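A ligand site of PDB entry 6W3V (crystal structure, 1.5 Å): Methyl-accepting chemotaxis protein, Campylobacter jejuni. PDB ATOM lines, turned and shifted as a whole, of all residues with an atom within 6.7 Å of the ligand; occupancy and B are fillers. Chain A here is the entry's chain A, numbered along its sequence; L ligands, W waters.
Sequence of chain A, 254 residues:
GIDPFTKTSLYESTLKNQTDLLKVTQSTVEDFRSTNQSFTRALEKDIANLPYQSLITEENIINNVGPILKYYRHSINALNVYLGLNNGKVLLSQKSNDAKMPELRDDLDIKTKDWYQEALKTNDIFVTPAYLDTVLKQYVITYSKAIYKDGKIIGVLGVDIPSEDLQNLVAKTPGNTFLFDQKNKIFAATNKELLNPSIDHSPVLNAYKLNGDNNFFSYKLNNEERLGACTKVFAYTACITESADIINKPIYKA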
ATOM      1  N   ASN A  80      24.968 -22.135  23.438  1.00  0.00           N
ATOM      2  CA  ASN A  80      23.752 -21.321  23.309  1.00  0.00           C
ATOM      3  C   ASN A  80      23.466 -21.173  21.834  1.00  0.00           C
ATOM      4  O   ASN A  80      24.389 -21.059  21.039  1.00  0.00           O
ATOM      5  CB  ASN A  80      23.960 -19.894  23.870  1.00  0.00           C
ATOM      6  CG  ASN A  80      24.271 -19.824  25.353  1.00  0.00           C
ATOM      7  OD1 ASN A  80      23.478 -20.260  26.199  1.00  0.00           O
ATOM      8  ND2 ASN A  80      25.451 -19.292  25.661  1.00  0.00           N
ATOM      9  N   TYR A  82      20.520 -18.703  19.635  1.00  0.00           N
ATOM     10  CA  TYR A  82      19.555 -17.686  19.935  1.00  0.00           C
ATOM     11  C   TYR A  82      19.226 -16.866  18.696  1.00  0.00           C
ATOM     12  O   TYR A  82      19.957 -16.780  17.725  1.00  0.00           O
ATOM     13  CB  TYR A  82      20.055 -16.789  21.072  1.00  0.00           C
ATOM     14  CG  TYR A  82      21.517 -16.380  21.003  1.00  0.00           C
ATOM     15  CD1 TYR A  82      22.509 -17.200  21.549  1.00  0.00           C
ATOM     16  CD2 TYR A  82      21.944 -15.238  20.346  1.00  0.00           C
ATOM     17  CE1 TYR A  82      23.827 -16.886  21.472  1.00  0.00           C
ATOM     18  CE2 TYR A  82      23.283 -14.917  20.244  1.00  0.00           C
ATOM     19  CZ  TYR A  82      24.235 -15.713  20.879  1.00  0.00           C
ATOM     20  OH  TYR A  82      25.552 -15.355  20.777  1.00  0.00           O
ATOM     21  N   VAL A  90      15.150 -11.591  22.801  1.00  0.00           N
ATOM     22  CA  VAL A  90      15.949 -12.663  22.219  1.00  0.00           C
ATOM     23  C   VAL A  90      15.360 -13.992  22.634  1.00  0.00           C
ATOM     24  O   VAL A  90      15.085 -14.242  23.834  1.00  0.00           O
ATOM     25  CB  VAL A  90      17.435 -12.557  22.567  1.00  0.00           C
ATOM     26  CG1 VAL A  90      17.646 -12.544  24.051  1.00  0.00           C
ATOM     27  CG2 VAL A  90      18.244 -13.684  21.939  1.00  0.00           C
ATOM     28  N   LEU A  91      15.209 -14.864  21.647  1.00  0.00           N
ATOM     29  CA  LEU A  91      14.804 -16.255  21.899  1.00  0.00           C
ATOM     30  C   LEU A  91      16.045 -17.058  22.148  1.00  0.00           C
ATOM     31  O   LEU A  91      16.910 -17.147  21.263  1.00  0.00           O
ATOM     32  CB  LEU A  91      14.026 -16.817  20.740  1.00  0.00           C
ATOM     33  CG  LEU A  91      13.485 -18.217  20.956  1.00  0.00           C
ATOM     34  CD1 LEU A  91      12.433 -18.251  22.053  1.00  0.00           C
ATOM     35  CD2 LEU A  91      12.949 -18.754  19.657  1.00  0.00           C
ATOM     36  N   LEU A  92      16.151 -17.571  23.371  1.00  0.00           N
ATOM     37  CA  LEU A  92      17.438 -18.158  23.817  1.00  0.00           C
ATOM     38  C   LEU A  92      17.261 -19.613  24.149  1.00  0.00           C
ATOM     39  O   LEU A  92      16.510 -19.980  25.036  1.00  0.00           O
ATOM     40  CB  LEU A  92      17.936 -17.392  25.057  1.00  0.00           C
ATOM     41  CG  LEU A  92      19.153 -17.896  25.779  1.00  0.00           C
ATOM     42  CD1 LEU A  92      20.381 -17.961  24.866  1.00  0.00           C
ATOM     43  CD2 LEU A  92      19.378 -17.034  27.013  1.00  0.00           C
ATOM     44  N   LEU A 108      18.205  -8.694  28.236  1.00  0.00           N
ATOM     45  CA  LEU A 108      19.579  -9.076  27.858  1.00  0.00           C
ATOM     46  C   LEU A 108      20.396  -8.085  26.970  1.00  0.00           C
ATOM     47  O   LEU A 108      21.537  -8.333  26.646  1.00  0.00           O
ATOM     48  CB  LEU A 108      19.566 -10.477  27.252  1.00  0.00           C
ATOM     49  CG  LEU A 108      19.333 -11.618  28.247  1.00  0.00           C
ATOM     50  CD1 LEU A 108      19.328 -12.958  27.539  1.00  0.00           C
ATOM     51  CD2 LEU A 108      20.391 -11.618  29.353  1.00  0.00           C
ATOM     52  N   ASP A 109      19.847  -6.917  26.651  1.00  0.00           N
ATOM     53  CA  ASP A 109      20.640  -5.782  26.094  1.00  0.00           C
ATOM     54  C   ASP A 109      21.342  -6.095  24.756  1.00  0.00           C
ATOM     55  O   ASP A 109      22.523  -5.753  24.559  1.00  0.00           O
ATOM     56  CB  ASP A 109      21.678  -5.283  27.109  1.00  0.00           C
ATOM     57  CG  ASP A 109      21.042  -4.802  28.407  1.00  0.00           C
ATOM     58  OD1 ASP A 109      20.099  -3.984  28.335  1.00  0.00           O
ATOM     59  OD2 ASP A 109      21.566  -5.173  29.484  1.00  0.00           O
ATOM     60  N   ILE A 110      20.612  -6.716  23.822  1.00  0.00           N
ATOM     61  CA  ILE A 110      21.241  -7.375  22.694  1.00  0.00           C
ATOM     62  C   ILE A 110      21.835  -6.411  21.704  1.00  0.00           C
ATOM     63  O   ILE A 110      22.767  -6.714  21.005  1.00  0.00           O
ATOM     64  CB  ILE A 110      20.318  -8.376  21.979  1.00  0.00           C
ATOM     65  CG1 ILE A 110      19.151  -7.670  21.289  1.00  0.00           C
ATOM     66  CG2 ILE A 110      19.846  -9.429  22.959  1.00  0.00           C
ATOM     67  CD1 ILE A 110      18.257  -8.596  20.505  1.00  0.00           C
ATOM     68  N   LYS A 113      25.594  -5.675  21.726  1.00  0.00           N
ATOM     69  CA  LYS A 113      26.530  -6.796  21.499  1.00  0.00           C
ATOM     70  C   LYS A 113      27.160  -6.687  20.113  1.00  0.00           C
ATOM     71  O   LYS A 113      26.501  -6.438  19.090  1.00  0.00           O
ATOM     72  CB  LYS A 113      25.811  -8.150  21.662  1.00  0.00           C
ATOM     73  CG  LYS A 113      25.099  -8.363  22.983  1.00  0.00           C
ATOM     74  CD  LYS A 113      26.071  -8.363  24.162  1.00  0.00           C
ATOM     75  CE  LYS A 113      25.392  -8.472  25.519  1.00  0.00           C
ATOM     76  NZ  LYS A 113      25.110  -9.859  25.891  1.00  0.00           N
ATOM     77  N   TRP A 115      28.199  -9.228  18.354  1.00  0.00           N
ATOM     78  CA  TRP A 115      27.637 -10.264  17.498  1.00  0.00           C
ATOM     79  C   TRP A 115      26.348  -9.795  16.826  1.00  0.00           C
ATOM     80  O   TRP A 115      26.053 -10.168  15.701  1.00  0.00           O
ATOM     81  CB  TRP A 115      27.451 -11.614  18.203  1.00  0.00           C
ATOM     82  CG  TRP A 115      26.480 -11.591  19.368  1.00  0.00           C
ATOM     83  CD1 TRP A 115      26.813 -11.605  20.683  1.00  0.00           C
ATOM     84  CD2 TRP A 115      25.042 -11.578  19.325  1.00  0.00           C
ATOM     85  NE1 TRP A 115      25.704 -11.599  21.458  1.00  0.00           N
ATOM     86  CE2 TRP A 115      24.595 -11.568  20.663  1.00  0.00           C
ATOM     87  CE3 TRP A 115      24.100 -11.665  18.309  1.00  0.00           C
ATOM     88  CZ2 TRP A 115      23.260 -11.533  20.997  1.00  0.00           C
ATOM     89  CZ3 TRP A 115      22.749 -11.648  18.660  1.00  0.00           C
ATOM     90  CH2 TRP A 115      22.349 -11.569  19.976  1.00  0.00           C
ATOM     91  N   TYR A 131      35.348 -14.704  23.736  1.00  0.00           N
ATOM     92  CA  TYR A 131      34.955 -13.784  24.822  1.00  0.00           C
ATOM     93  C   TYR A 131      34.116 -14.570  25.832  1.00  0.00           C
ATOM     94  O   TYR A 131      33.625 -15.669  25.527  1.00  0.00           O
ATOM     95  CB  TYR A 131      34.165 -12.584  24.274  1.00  0.00           C
ATOM     96  CG  TYR A 131      32.816 -12.993  23.779  1.00  0.00           C
ATOM     97  CD1 TYR A 131      32.633 -13.468  22.483  1.00  0.00           C
ATOM     98  CD2 TYR A 131      31.696 -12.767  24.564  1.00  0.00           C
ATOM     99  CE1 TYR A 131      31.368 -13.866  22.044  1.00  0.00           C
ATOM    100  CE2 TYR A 131      30.458 -13.175  24.157  1.00  0.00           C
ATOM    101  CZ  TYR A 131      30.285 -13.712  22.894  1.00  0.00           C
ATOM    102  OH  TYR A 131      29.041 -14.110  22.509  1.00  0.00           O
ATOM    103  N   LEU A 132      33.977 -14.005  27.035  1.00  0.00           N
ATOM    104  CA  LEU A 132      33.150 -14.603  28.077  1.00  0.00           C
ATOM    105  C   LEU A 132      31.642 -14.427  27.842  1.00  0.00           C
ATOM    106  O   LEU A 132      31.113 -13.331  27.966  1.00  0.00           O
ATOM    107  CB  LEU A 132      33.495 -14.036  29.449  1.00  0.00           C
ATOM    108  CG  LEU A 132      32.943 -14.770  30.680  1.00  0.00           C
ATOM    109  CD1 LEU A 132      33.517 -16.200  30.737  1.00  0.00           C
ATOM    110  CD2 LEU A 132      33.207 -14.011  31.984  1.00  0.00           C
ATOM    111  N   ASP A 133      30.962 -15.528  27.580  1.00  0.00           N
ATOM    112  CA  ASP A 133      29.503 -15.520  27.425  1.00  0.00           C
ATOM    113  C   ASP A 133      28.900 -15.107  28.737  1.00  0.00           C
ATOM    114  O   ASP A 133      29.164 -15.713  29.790  1.00  0.00           O
ATOM    115  CB  ASP A 133      29.064 -16.934  27.088  1.00  0.00           C
ATOM    116  CG  ASP A 133      27.594 -17.143  27.215  1.00  0.00           C
ATOM    117  OD1 ASP A 133      26.854 -16.250  26.743  1.00  0.00           O
ATOM    118  OD2 ASP A 133      27.194 -18.179  27.834  1.00  0.00           O
ATOM    119  N   THR A 134      27.921 -14.195  28.624  1.00  0.00           N
ATOM    120  CA  THR A 134      27.265 -13.716  29.833  1.00  0.00           C
ATOM    121  C   THR A 134      26.175 -14.664  30.352  1.00  0.00           C
ATOM    122  O   THR A 134      25.795 -14.591  31.527  1.00  0.00           O
ATOM    123  CB  THR A 134      26.649 -12.318  29.652  1.00  0.00           C
ATOM    124  OG1 THR A 134      25.704 -12.383  28.588  1.00  0.00           O
ATOM    125  CG2 THR A 134      27.740 -11.321  29.288  1.00  0.00           C
ATOM    126  N   VAL A 135      25.650 -15.503  29.475  1.00  0.00           N
ATOM    127  CA  VAL A 135      24.557 -16.405  29.869  1.00  0.00           C
ATOM    128  C   VAL A 135      25.111 -17.540  30.759  1.00  0.00           C
ATOM    129  O   VAL A 135      24.665 -17.754  31.885  1.00  0.00           O
ATOM    130  CB  VAL A 135      23.793 -16.956  28.649  1.00  0.00           C
ATOM    131  CG1 VAL A 135      22.804 -18.026  29.088  1.00  0.00           C
ATOM    132  CG2 VAL A 135      23.039 -15.840  27.928  1.00  0.00           C
ATOM    133  N   LEU A 136      26.156 -18.215  30.283  1.00  0.00           N
ATOM    134  CA  LEU A 136      26.666 -19.391  30.969  1.00  0.00           C
ATOM    135  C   LEU A 136      28.109 -19.194  31.490  1.00  0.00           C
ATOM    136  O   LEU A 136      28.661 -20.078  32.120  1.00  0.00           O
ATOM    137  CB  LEU A 136      26.530 -20.671  30.094  1.00  0.00           C
ATOM    138  CG  LEU A 136      25.086 -21.235  29.951  1.00  0.00           C
ATOM    139  CD1 LEU A 136      24.903 -22.268  28.839  1.00  0.00           C
ATOM    140  CD2 LEU A 136      24.541 -21.763  31.280  1.00  0.00           C
ATOM    141  N   GLN A 138      31.098 -19.057  30.186  1.00  0.00           N
ATOM    142  CA  GLN A 138      32.220 -19.750  29.542  1.00  0.00           C
ATOM    143  C   GLN A 138      32.764 -18.941  28.381  1.00  0.00           C
ATOM    144  O   GLN A 138      32.004 -18.248  27.702  1.00  0.00           O
ATOM    145  CB  GLN A 138      31.827 -21.155  29.070  1.00  0.00           C
ATOM    146  CG  GLN A 138      31.249 -21.992  30.188  1.00  0.00           C
ATOM    147  CD  GLN A 138      30.825 -23.355  29.728  1.00  0.00           C
ATOM    148  OE1 GLN A 138      31.387 -23.874  28.767  1.00  0.00           O
ATOM    149  NE2 GLN A 138      29.784 -23.908  30.339  1.00  0.00           N
ATOM    150  N   VAL A 140      33.556 -18.332  24.656  1.00  0.00           N
ATOM    151  CA  VAL A 140      32.902 -18.812  23.458  1.00  0.00           C
ATOM    152  C   VAL A 140      33.403 -18.059  22.249  1.00  0.00           C
ATOM    153  O   VAL A 140      33.922 -16.962  22.371  1.00  0.00           O
ATOM    154  CB  VAL A 140      31.376 -18.724  23.493  1.00  0.00           C
ATOM    155  CG1 VAL A 140      30.786 -19.528  24.634  1.00  0.00           C
ATOM    156  CG2 VAL A 140      30.912 -17.277  23.542  1.00  0.00           C
ATOM    157  N   THR A 142      31.423 -16.866  18.866  1.00  0.00           N
ATOM    158  CA  THR A 142      30.040 -16.723  18.390  1.00  0.00           C
ATOM    159  C   THR A 142      30.035 -16.540  16.889  1.00  0.00           C
ATOM    160  O   THR A 142      30.816 -15.776  16.335  1.00  0.00           O
ATOM    161  CB  THR A 142      29.358 -15.534  19.064  1.00  0.00           C
ATOM    162  OG1 THR A 142      29.267 -15.778  20.480  1.00  0.00           O
ATOM    163  CG2 THR A 142      27.958 -15.278  18.516  1.00  0.00           C
ATOM    164  N   ASP A 160      26.828 -20.052  19.866  1.00  0.00           N
ATOM    165  CA  ASP A 160      28.019 -19.993  20.746  1.00  0.00           C
ATOM    166  C   ASP A 160      28.628 -21.377  20.848  1.00  0.00           C
ATOM    167  O   ASP A 160      27.982 -22.314  21.337  1.00  0.00           O
ATOM    168  CB  ASP A 160      27.639 -19.553  22.160  1.00  0.00           C
ATOM    169  CG  ASP A 160      27.123 -18.118  22.249  1.00  0.00           C
ATOM    170  OD1 ASP A 160      27.268 -17.344  21.273  1.00  0.00           O
ATOM    171  OD2 ASP A 160      26.631 -17.797  23.348  1.00  0.00           O
HETATM  172  N1  LIG L   1      27.199 -15.316  24.232  1.00  0.00           N
HETATM  173  C1  LIG L   1      26.137 -14.287  24.109  1.00  0.00           C
HETATM  174  C2  LIG L   1      26.636 -13.005  24.746  1.00  0.00           C
HETATM  175  O1  LIG L   1      27.289 -13.087  25.796  1.00  0.00           O
HETATM  176  C3  LIG L   1      24.890 -14.776  24.865  1.00  0.00           C
HETATM  177  C4  LIG L   1      23.730 -13.859  24.775  1.00  0.00           C
HETATM  178  C5  LIG L   1      23.646 -12.812  25.632  1.00  0.00           C
HETATM  179  C6  LIG L   1      22.725 -14.087  23.882  1.00  0.00           C
HETATM  180  C7  LIG L   1      22.546 -11.989  25.622  1.00  0.00           C
HETATM  181  C8  LIG L   1      21.662 -13.239  23.830  1.00  0.00           C
HETATM  182  C9  LIG L   1      21.637 -12.127  24.636  1.00  0.00           C
HETATM  183  O2  LIG L   1      26.357 -11.912  24.212  1.00  0.00           O
HETATM  184  O   HOH W   1      28.403 -10.489  26.201  1.00  0.00           O
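Residues that only touch the ligand: Tyr 82 (3.5 Å), Ile 110 (3.6 Å), Leu 108 (3.7 Å), Val 135 (3.7 Å) and Val 90 (3.9 Å). Hydrophobic or aromatic side chains within 4 Å of the ligand: Tyr 82, Val 90, Leu 108, Ile 110, Trp 115, Tyr 131 and Val 135. Of the 20 residues printed, 11 come within 4 Å of the ligand.
Water W1 lies within hydrogen-bond range of an oxygen (O1) of the ligand (2.9 Å) and the side-chain amino group of Lys 113 (3.4 Å).
A nitrogen (N1) of the ligand is in salt-bridge range of the side-chain carboxylate (OD2) of Asp 160 (2.7 Å). The side-chain hydroxyl (OG1) of Thr 134 sits at hydrogen-bond distance from an oxygen (O1) of the ligand (3.3 Å). N of Thr 134 sits at hydrogen-bond distance from O1 of the ligand, 3.1 Å away. The side-chain hydroxyl (OH) of Tyr 131 sits at hydrogen-bond distance from a nitrogen (N1) of the ligand (2.8 Å). The side-chain amino group (NZ) of Lys 113 is in salt-bridge range of an oxygen (O2) of the ligand (2.9 Å). N1 of the ligand lies within salt-bridge range of OD1 of Asp 133 (2.7 Å). The indole nitrogen (NE1) of Trp 115 is in hydrogen-bond range of an oxygen (O2) of the ligand (2.8 Å).
N of Asp 160 is in hydrogen-bond range of O of Asn 80 (2.9 Å). The side-chain carboxylate of Asp 133 sits at hydrogen-bond distance from the backbone NH of Val 135, at 3.1 Å. The backbone NH (N) of Leu 136 sits at hydrogen-bond distance from the side-chain carboxylate (OD2) of Asp 133 (2.7 Å). OD1 of Asp 160 sits at hydrogen-bond distance from OG1 of Thr 142 (2.7 Å). The side-chain hydroxyl (OH) of Tyr 131 is in hydrogen-bond range of the side-chain hydroxyl (OG1) of Thr 142, at 2.6 Å. The backbone NH of Asp 133 sits at hydrogen-bond distance from the backbone carbonyl oxygen of Gln 138 (2.9 Å). OH of Tyr 82 lies within hydrogen-bond range of OD1 of Asp 160 (2.7 Å). The side-chain carboxylate (OD2) of Asp 133 lies within hydrogen-bond range of the side-chain amide nitrogen (ND2) of Asn 80 (3.0 Å).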
